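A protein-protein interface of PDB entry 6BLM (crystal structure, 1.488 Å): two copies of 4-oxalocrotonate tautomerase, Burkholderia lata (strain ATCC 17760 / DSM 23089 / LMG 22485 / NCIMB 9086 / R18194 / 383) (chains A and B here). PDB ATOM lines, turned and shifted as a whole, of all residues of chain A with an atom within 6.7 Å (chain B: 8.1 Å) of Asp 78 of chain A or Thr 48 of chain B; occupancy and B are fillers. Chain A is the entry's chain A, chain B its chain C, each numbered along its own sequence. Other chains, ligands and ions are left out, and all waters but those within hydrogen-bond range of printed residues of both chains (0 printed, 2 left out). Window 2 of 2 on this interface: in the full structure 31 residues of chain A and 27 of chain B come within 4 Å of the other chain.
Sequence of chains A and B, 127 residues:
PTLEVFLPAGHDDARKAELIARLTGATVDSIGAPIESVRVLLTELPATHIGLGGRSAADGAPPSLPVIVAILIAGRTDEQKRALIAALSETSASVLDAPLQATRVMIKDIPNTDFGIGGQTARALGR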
ATOM      1  N   ARG A  76      -2.599 -11.248  20.650  1.00  0.00           N
ATOM      2  CA  ARG A  76      -2.646 -10.764  19.281  1.00  0.00           C
ATOM      3  C   ARG A  76      -1.353 -10.028  18.966  1.00  0.00           C
ATOM      4  O   ARG A  76      -0.816  -9.308  19.814  1.00  0.00           O
ATOM      5  CB  ARG A  76      -3.855  -9.848  19.059  1.00  0.00           C
ATOM      6  CG  ARG A  76      -5.135 -10.572  18.685  1.00  0.00           C
ATOM      7  CD  ARG A  76      -5.551 -11.576  19.746  1.00  0.00           C
ATOM      8  NE  ARG A  76      -6.701 -12.381  19.328  1.00  0.00           N
ATOM      9  CZ  ARG A  76      -7.810 -12.541  20.047  1.00  0.00           C
ATOM     10  NH1 ARG A  76      -8.801 -13.290  19.578  1.00  0.00           N
ATOM     11  NH2 ARG A  76      -7.931 -11.963  21.235  1.00  0.00           N
ATOM     12  N   THR A  77      -0.847 -10.206  17.750  1.00  0.00           N
ATOM     13  CA  THR A  77       0.387  -9.545  17.357  1.00  0.00           C
ATOM     14  C   THR A  77       0.180  -8.069  17.054  1.00  0.00           C
ATOM     15  O   THR A  77      -0.955  -7.602  16.911  1.00  0.00           O
ATOM     16  CB  THR A  77       1.004 -10.204  16.121  1.00  0.00           C
ATOM     17  OG1 THR A  77       0.191  -9.928  14.976  1.00  0.00           O
ATOM     18  CG2 THR A  77       1.111 -11.707  16.328  1.00  0.00           C
ATOM     19  N   ASP A  78       1.284  -7.333  16.951  1.00  0.00           N
ATOM     20  CA  ASP A  78       1.210  -5.926  16.594  1.00  0.00           C
ATOM     21  C   ASP A  78       0.551  -5.773  15.231  1.00  0.00           C
ATOM     22  O   ASP A  78      -0.253  -4.870  15.023  1.00  0.00           O
ATOM     23  CB  ASP A  78       2.605  -5.278  16.593  1.00  0.00           C
ATOM     24  CG  ASP A  78       3.174  -5.095  17.992  1.00  0.00           C
ATOM     25  OD1 ASP A  78       2.435  -5.284  18.977  1.00  0.00           O
ATOM     26  OD2 ASP A  78       4.370  -4.736  18.112  1.00  0.00           O
ATOM     27  N   GLU A  79       0.875  -6.662  14.294  1.00  0.00           N
ATOM     28  CA  GLU A  79       0.235  -6.614  12.982  1.00  0.00           C
ATOM     29  C   GLU A  79      -1.269  -6.871  13.075  1.00  0.00           C
ATOM     30  O   GLU A  79      -2.055  -6.221  12.383  1.00  0.00           O
ATOM     31  CB  GLU A  79       0.888  -7.625  12.024  1.00  0.00           C
ATOM     32  CG  GLU A  79       0.123  -7.861  10.719  1.00  0.00           C
ATOM     33  CD  GLU A  79      -0.088  -6.594   9.906  1.00  0.00           C
ATOM     34  OE1 GLU A  79       0.798  -5.709   9.929  1.00  0.00           O
ATOM     35  OE2 GLU A  79      -1.144  -6.488   9.239  1.00  0.00           O
ATOM     36  N   GLN A  80      -1.682  -7.819  13.916  1.00  0.00           N
ATOM     37  CA  GLN A  80      -3.112  -8.082  14.067  1.00  0.00           C
ATOM     38  C   GLN A  80      -3.796  -6.842  14.629  1.00  0.00           C
ATOM     39  O   GLN A  80      -4.877  -6.475  14.199  1.00  0.00           O
ATOM     40  CB  GLN A  80      -3.365  -9.268  14.985  1.00  0.00           C
ATOM     41  CG  GLN A  80      -3.023 -10.628  14.379  1.00  0.00           C
ATOM     42  CD  GLN A  80      -3.316 -11.729  15.362  1.00  0.00           C
ATOM     43  OE1 GLN A  80      -2.563 -11.927  16.307  1.00  0.00           O
ATOM     44  NE2 GLN A  80      -4.432 -12.429  15.171  1.00  0.00           N
ATOM     45  N   LYS A  81      -3.141  -6.206  15.583  1.00  0.00           N
ATOM     46  CA  LYS A  81      -3.711  -5.021  16.215  1.00  0.00           C
ATOM     47  C   LYS A  81      -3.790  -3.867  15.218  1.00  0.00           C
ATOM     48  O   LYS A  81      -4.775  -3.113  15.208  1.00  0.00           O
ATOM     49  CB  LYS A  81      -2.895  -4.648  17.448  1.00  0.00           C
ATOM     50  CG  LYS A  81      -3.093  -5.642  18.571  1.00  0.00           C
ATOM     51  CD  LYS A  81      -2.160  -5.401  19.728  1.00  0.00           C
ATOM     52  CE  LYS A  81      -2.484  -6.361  20.858  1.00  0.00           C
ATOM     53  NZ  LYS A  81      -1.384  -6.382  21.842  1.00  0.00           N
ATOM     54  N   ARG A  82      -2.770  -3.729  14.372  1.00  0.00           N
ATOM     55  CA  ARG A  82      -2.788  -2.709  13.336  1.00  0.00           C
ATOM     56  C   ARG A  82      -3.970  -2.933  12.401  1.00  0.00           C
ATOM     57  O   ARG A  82      -4.688  -1.995  12.056  1.00  0.00           O
ATOM     58  CB  ARG A  82      -1.460  -2.708  12.561  1.00  0.00           C
ATOM     59  CG  ARG A  82      -1.342  -1.653  11.483  1.00  0.00           C
ATOM     60  CD  ARG A  82       0.015  -1.741  10.786  1.00  0.00           C
ATOM     61  NE  ARG A  82      -0.017  -2.627   9.626  1.00  0.00           N
ATOM     62  CZ  ARG A  82       0.864  -2.587   8.631  1.00  0.00           C
ATOM     63  NH1 ARG A  82       1.852  -1.700   8.649  1.00  0.00           N
ATOM     64  NH2 ARG A  82       0.758  -3.432   7.613  1.00  0.00           N
ATOM     65  N   ALA A  83      -4.180  -4.183  11.984  1.00  0.00           N
ATOM     66  CA  ALA A  83      -5.291  -4.497  11.107  1.00  0.00           C
ATOM     67  C   ALA A  83      -6.627  -4.194  11.777  1.00  0.00           C
ATOM     68  O   ALA A  83      -7.538  -3.673  11.142  1.00  0.00           O
ATOM     69  CB  ALA A  83      -5.240  -5.969  10.677  1.00  0.00           C
ATOM     70  N   ILE A  85      -7.253  -2.027  14.219  1.00  0.00           N
ATOM     71  CA  ILE A  85      -7.449  -0.585  14.306  1.00  0.00           C
ATOM     72  C   ILE A  85      -7.928  -0.022  12.975  1.00  0.00           C
ATOM     73  O   ILE A  85      -8.873   0.756  12.920  1.00  0.00           O
ATOM     74  CB  ILE A  85      -6.152   0.105  14.750  1.00  0.00           C
ATOM     75  CG1 ILE A  85      -5.910  -0.163  16.245  1.00  0.00           C
ATOM     76  CG2 ILE A  85      -6.176   1.608  14.449  1.00  0.00           C
ATOM     77  CD1 ILE A  85      -4.519   0.218  16.710  1.00  0.00           C
ATOM     78  N   ILE A 107      -7.171  -0.389  22.383  1.00  0.00           N
ATOM     79  CA  ILE A 107      -7.154  -1.822  22.638  1.00  0.00           C
ATOM     80  C   ILE A 107      -6.645  -2.119  24.036  1.00  0.00           C
ATOM     81  O   ILE A 107      -5.582  -1.634  24.427  1.00  0.00           O
ATOM     82  CB  ILE A 107      -6.272  -2.549  21.629  1.00  0.00           C
ATOM     83  CG1 ILE A 107      -6.801  -2.342  20.212  1.00  0.00           C
ATOM     84  CG2 ILE A 107      -6.220  -4.040  21.957  1.00  0.00           C
ATOM     85  CD1 ILE A 107      -5.810  -2.771  19.102  1.00  0.00           C
ATOM     86  N   ALA B   9       1.496   5.364  26.789  1.00  0.00           N
ATOM     87  CA  ALA B   9       2.634   5.102  27.660  1.00  0.00           C
ATOM     88  C   ALA B   9       3.750   6.123  27.433  1.00  0.00           C
ATOM     89  O   ALA B   9       3.851   6.727  26.358  1.00  0.00           O
ATOM     90  CB  ALA B   9       3.147   3.681  27.439  1.00  0.00           C
ATOM     91  N   LEU B  45      -1.731   2.737  27.777  1.00  0.00           N
ATOM     92  CA  LEU B  45      -1.682   1.815  26.648  1.00  0.00           C
ATOM     93  C   LEU B  45      -0.445   2.032  25.802  1.00  0.00           C
ATOM     94  O   LEU B  45      -0.039   3.162  25.568  1.00  0.00           O
ATOM     95  CB  LEU B  45      -2.930   1.972  25.777  1.00  0.00           C
ATOM     96  CG  LEU B  45      -4.261   1.686  26.473  1.00  0.00           C
ATOM     97  CD1 LEU B  45      -5.368   1.879  25.459  1.00  0.00           C
ATOM     98  CD2 LEU B  45      -4.306   0.281  27.039  1.00  0.00           C
ATOM     99  N   PRO B  46       0.153   0.935  25.333  1.00  0.00           N
ATOM    100  CA  PRO B  46       1.241   1.063  24.362  1.00  0.00           C
ATOM    101  C   PRO B  46       0.758   1.731  23.083  1.00  0.00           C
ATOM    102  O   PRO B  46      -0.427   1.653  22.772  1.00  0.00           O
ATOM    103  CB  PRO B  46       1.650  -0.391  24.083  1.00  0.00           C
ATOM    104  CG  PRO B  46       1.032  -1.204  25.167  1.00  0.00           C
ATOM    105  CD  PRO B  46      -0.196  -0.464  25.611  1.00  0.00           C
ATOM    106  N   ALA B  47       1.660   2.360  22.339  1.00  0.00           N
ATOM    107  CA  ALA B  47       1.301   3.051  21.103  1.00  0.00           C
ATOM    108  C   ALA B  47       0.657   2.109  20.081  1.00  0.00           C
ATOM    109  O   ALA B  47      -0.168   2.524  19.264  1.00  0.00           O
ATOM    110  CB  ALA B  47       2.538   3.721  20.501  1.00  0.00           C
ATOM    111  N   THR B  48       1.026   0.841  20.139  1.00  0.00           N
ATOM    112  CA  THR B  48       0.457  -0.159  19.242  1.00  0.00           C
ATOM    113  C   THR B  48      -1.005  -0.488  19.553  1.00  0.00           C
ATOM    114  O   THR B  48      -1.641  -1.235  18.799  1.00  0.00           O
ATOM    115  CB  THR B  48       1.247  -1.455  19.302  1.00  0.00           C
ATOM    116  OG1 THR B  48       1.424  -1.843  20.667  1.00  0.00           O
ATOM    117  CG2 THR B  48       2.621  -1.292  18.626  1.00  0.00           C
ATOM    118  N   HIS B  49      -1.519   0.041  20.664  1.00  0.00           N
ATOM    119  CA  HIS B  49      -2.906  -0.197  21.076  1.00  0.00           C
ATOM    120  C   HIS B  49      -3.807   0.981  20.819  1.00  0.00           C
ATOM    121  O   HIS B  49      -5.006   0.942  21.111  1.00  0.00           O
ATOM    122  CB  HIS B  49      -2.996  -0.518  22.564  1.00  0.00           C
ATOM    123  CG  HIS B  49      -2.471  -1.862  22.929  1.00  0.00           C
ATOM    124  ND1 HIS B  49      -2.943  -2.565  24.011  1.00  0.00           N
ATOM    125  CD2 HIS B  49      -1.499  -2.627  22.376  1.00  0.00           C
ATOM    126  CE1 HIS B  49      -2.292  -3.712  24.110  1.00  0.00           C
ATOM    127  NE2 HIS B  49      -1.410  -3.773  23.128  1.00  0.00           N
ATOM    128  N   ILE B  50      -3.238   2.052  20.303  1.00  0.00           N
ATOM    129  CA  ILE B  50      -3.978   3.282  20.197  1.00  0.00           C
ATOM    130  C   ILE B  50      -4.107   3.652  18.737  1.00  0.00           C
ATOM    131  O   ILE B  50      -3.100   3.798  18.030  1.00  0.00           O
ATOM    132  CB  ILE B  50      -3.307   4.408  20.992  1.00  0.00           C
ATOM    133  CG1 ILE B  50      -3.183   4.004  22.464  1.00  0.00           C
ATOM    134  CG2 ILE B  50      -4.099   5.688  20.855  1.00  0.00           C
ATOM    135  CD1 ILE B  50      -2.529   5.060  23.344  1.00  0.00           C
ATOM    136  N   GLY B  51      -5.347   3.768  18.281  1.00  0.00           N
ATOM    137  CA  GLY B  51      -5.620   4.167  16.912  1.00  0.00           C
ATOM    138  C   GLY B  51      -6.178   5.572  16.854  1.00  0.00           C
ATOM    139  O   GLY B  51      -7.069   5.939  17.629  1.00  0.00           O
ATOM    140  N   ARG B  55      -5.086   4.562  12.155  1.00  0.00           N
ATOM    141  CA  ARG B  55      -3.707   4.096  12.302  1.00  0.00           C
ATOM    142  C   ARG B  55      -3.197   4.301  13.719  1.00  0.00           C
ATOM    143  O   ARG B  55      -3.653   5.202  14.413  1.00  0.00           O
ATOM    144  CB  ARG B  55      -2.758   4.836  11.343  1.00  0.00           C
ATOM    145  CG  ARG B  55      -3.323   5.195   9.987  1.00  0.00           C
ATOM    146  CD  ARG B  55      -2.613   4.446   8.870  1.00  0.00           C
ATOM    147  NE  ARG B  55      -2.542   5.248   7.649  1.00  0.00           N
ATOM    148  CZ  ARG B  55      -2.137   4.787   6.470  1.00  0.00           C
ATOM    149  NH1 ARG B  55      -1.773   3.518   6.338  1.00  0.00           N
ATOM    150  NH2 ARG B  55      -2.103   5.594   5.417  1.00  0.00           N
ATOM    151  N   SER B  56      -2.205   3.501  14.111  1.00  0.00           N
ATOM    152  CA  SER B  56      -1.448   3.740  15.338  1.00  0.00           C
ATOM    153  C   SER B  56      -0.356   4.775  15.082  1.00  0.00           C
ATOM    154  O   SER B  56      -0.054   5.058  13.934  1.00  0.00           O
ATOM    155  CB  SER B  56      -0.827   2.441  15.848  1.00  0.00           C
ATOM    156  OG  SER B  56      -0.001   1.855  14.852  1.00  0.00           O
ATOM    157  N   ALA B  57       0.222   5.344  16.140  1.00  0.00           N
ATOM    158  CA  ALA B  57       1.356   6.263  15.988  1.00  0.00           C
ATOM    159  C   ALA B  57       2.466   5.606  15.174  1.00  0.00           C
ATOM    160  O   ALA B  57       3.095   6.240  14.311  1.00  0.00           O
ATOM    161  CB  ALA B  57       1.882   6.698  17.352  1.00  0.00           C
ATOM    162  N   ALA B  58       2.674   4.320  15.444  1.00  0.00           N
ATOM    163  CA  ALA B  58       3.685   3.522  14.770  1.00  0.00           C
ATOM    164  C   ALA B  58       3.458   3.460  13.267  1.00  0.00           C
ATOM    165  O   ALA B  58       4.393   3.221  12.502  1.00  0.00           O
ATOM    166  CB  ALA B  58       3.711   2.112  15.357  1.00  0.00           C
ATOM    167  N   ASP B  59       2.218   3.674  12.839  1.00  0.00           N
ATOM    168  CA  ASP B  59       1.912   3.652  11.417  1.00  0.00           C
ATOM    169  C   ASP B  59       1.617   5.053  10.874  1.00  0.00           C
ATOM    170  O   ASP B  59       1.115   5.207   9.761  1.00  0.00           O
ATOM    171  CB  ASP B  59       0.738   2.717  11.130  1.00  0.00           C
ATOM    172  CG  ASP B  59       0.947   1.904   9.870  1.00  0.00           C
ATOM    173  OD1 ASP B  59       1.968   2.124   9.180  1.00  0.00           O
ATOM    174  OD2 ASP B  59       0.094   1.052   9.560  1.00  0.00           O
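Of the 10 printed residues of chain A, 5 touch a printed residue of chain B. Of the 13 printed residues of chain B, 6 touch a printed residue of chain A. Hydrophobic or aromatic side chains of chain B that line the printed part of chain A: Leu 45 and His 49. Among the printed residues, 9 pairs touch across the chains.
OE1 of Glu 79 of chain A is in salt-bridge range of NE of Arg 82 of chain A, at 3.2 Å. The backbone NH (N) of Ala 9 of chain B sits at hydrogen-bond distance from the backbone carbonyl oxygen (O) of Leu 45 of chain B (2.9 Å).
ND1 of His 49 of chain B is in hydrogen-bond range of O of Ile 107 of chain A (2.8 Å). A ring nitrogen (NE2) of His 49 of chain B is in hydrogen-bond range of the side-chain amino group (NZ) of Lys 81 of chain A, 2.9 Å away. The guanidinium group of Arg 82 of chain A lies within salt-bridge range of the side-chain carboxylate of Asp 59 of chain B.
CG of Asp 78 of chain A touches CG2 of Thr 48 of chain B, 3.9 Å away. Thr 48 of chain B touches Lys 81 of chain A. Ile 85 of chain A touches Thr 48 of chain B (CD1 to O, 3.8 Å). Gly 51 of chain B touches Ile 85 of chain A (CA to CG2, 3.6 Å). N of Arg 55 of chain B touches CG2 of Ile 85 of chain A, at 3.9 Å. Leu 45 of chain B touches Ile 107 of chain A (CD2 to O, 3.5 Å).
Gln 80 of chain A touches none of the printed residues of chain B. Printed residues of chain B within 4 Å of Lys 81 of chain A: Thr 48 and His 49. Of the printed residues of chain B, Ile 107 of chain A touches Leu 45 and His 49. Ile 50 of chain B touches none of the printed residues of chain A. Of the printed residues of chain A, Arg 55 of chain B touches Ile 85. Of the printed residues of chain A, Asp 59 of chain B touches Arg 82. The nearest residue of chain B that does not touch Asp 78 of chain A is His 49 of chain B (5.8 Å).
No position is printed for both chains.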
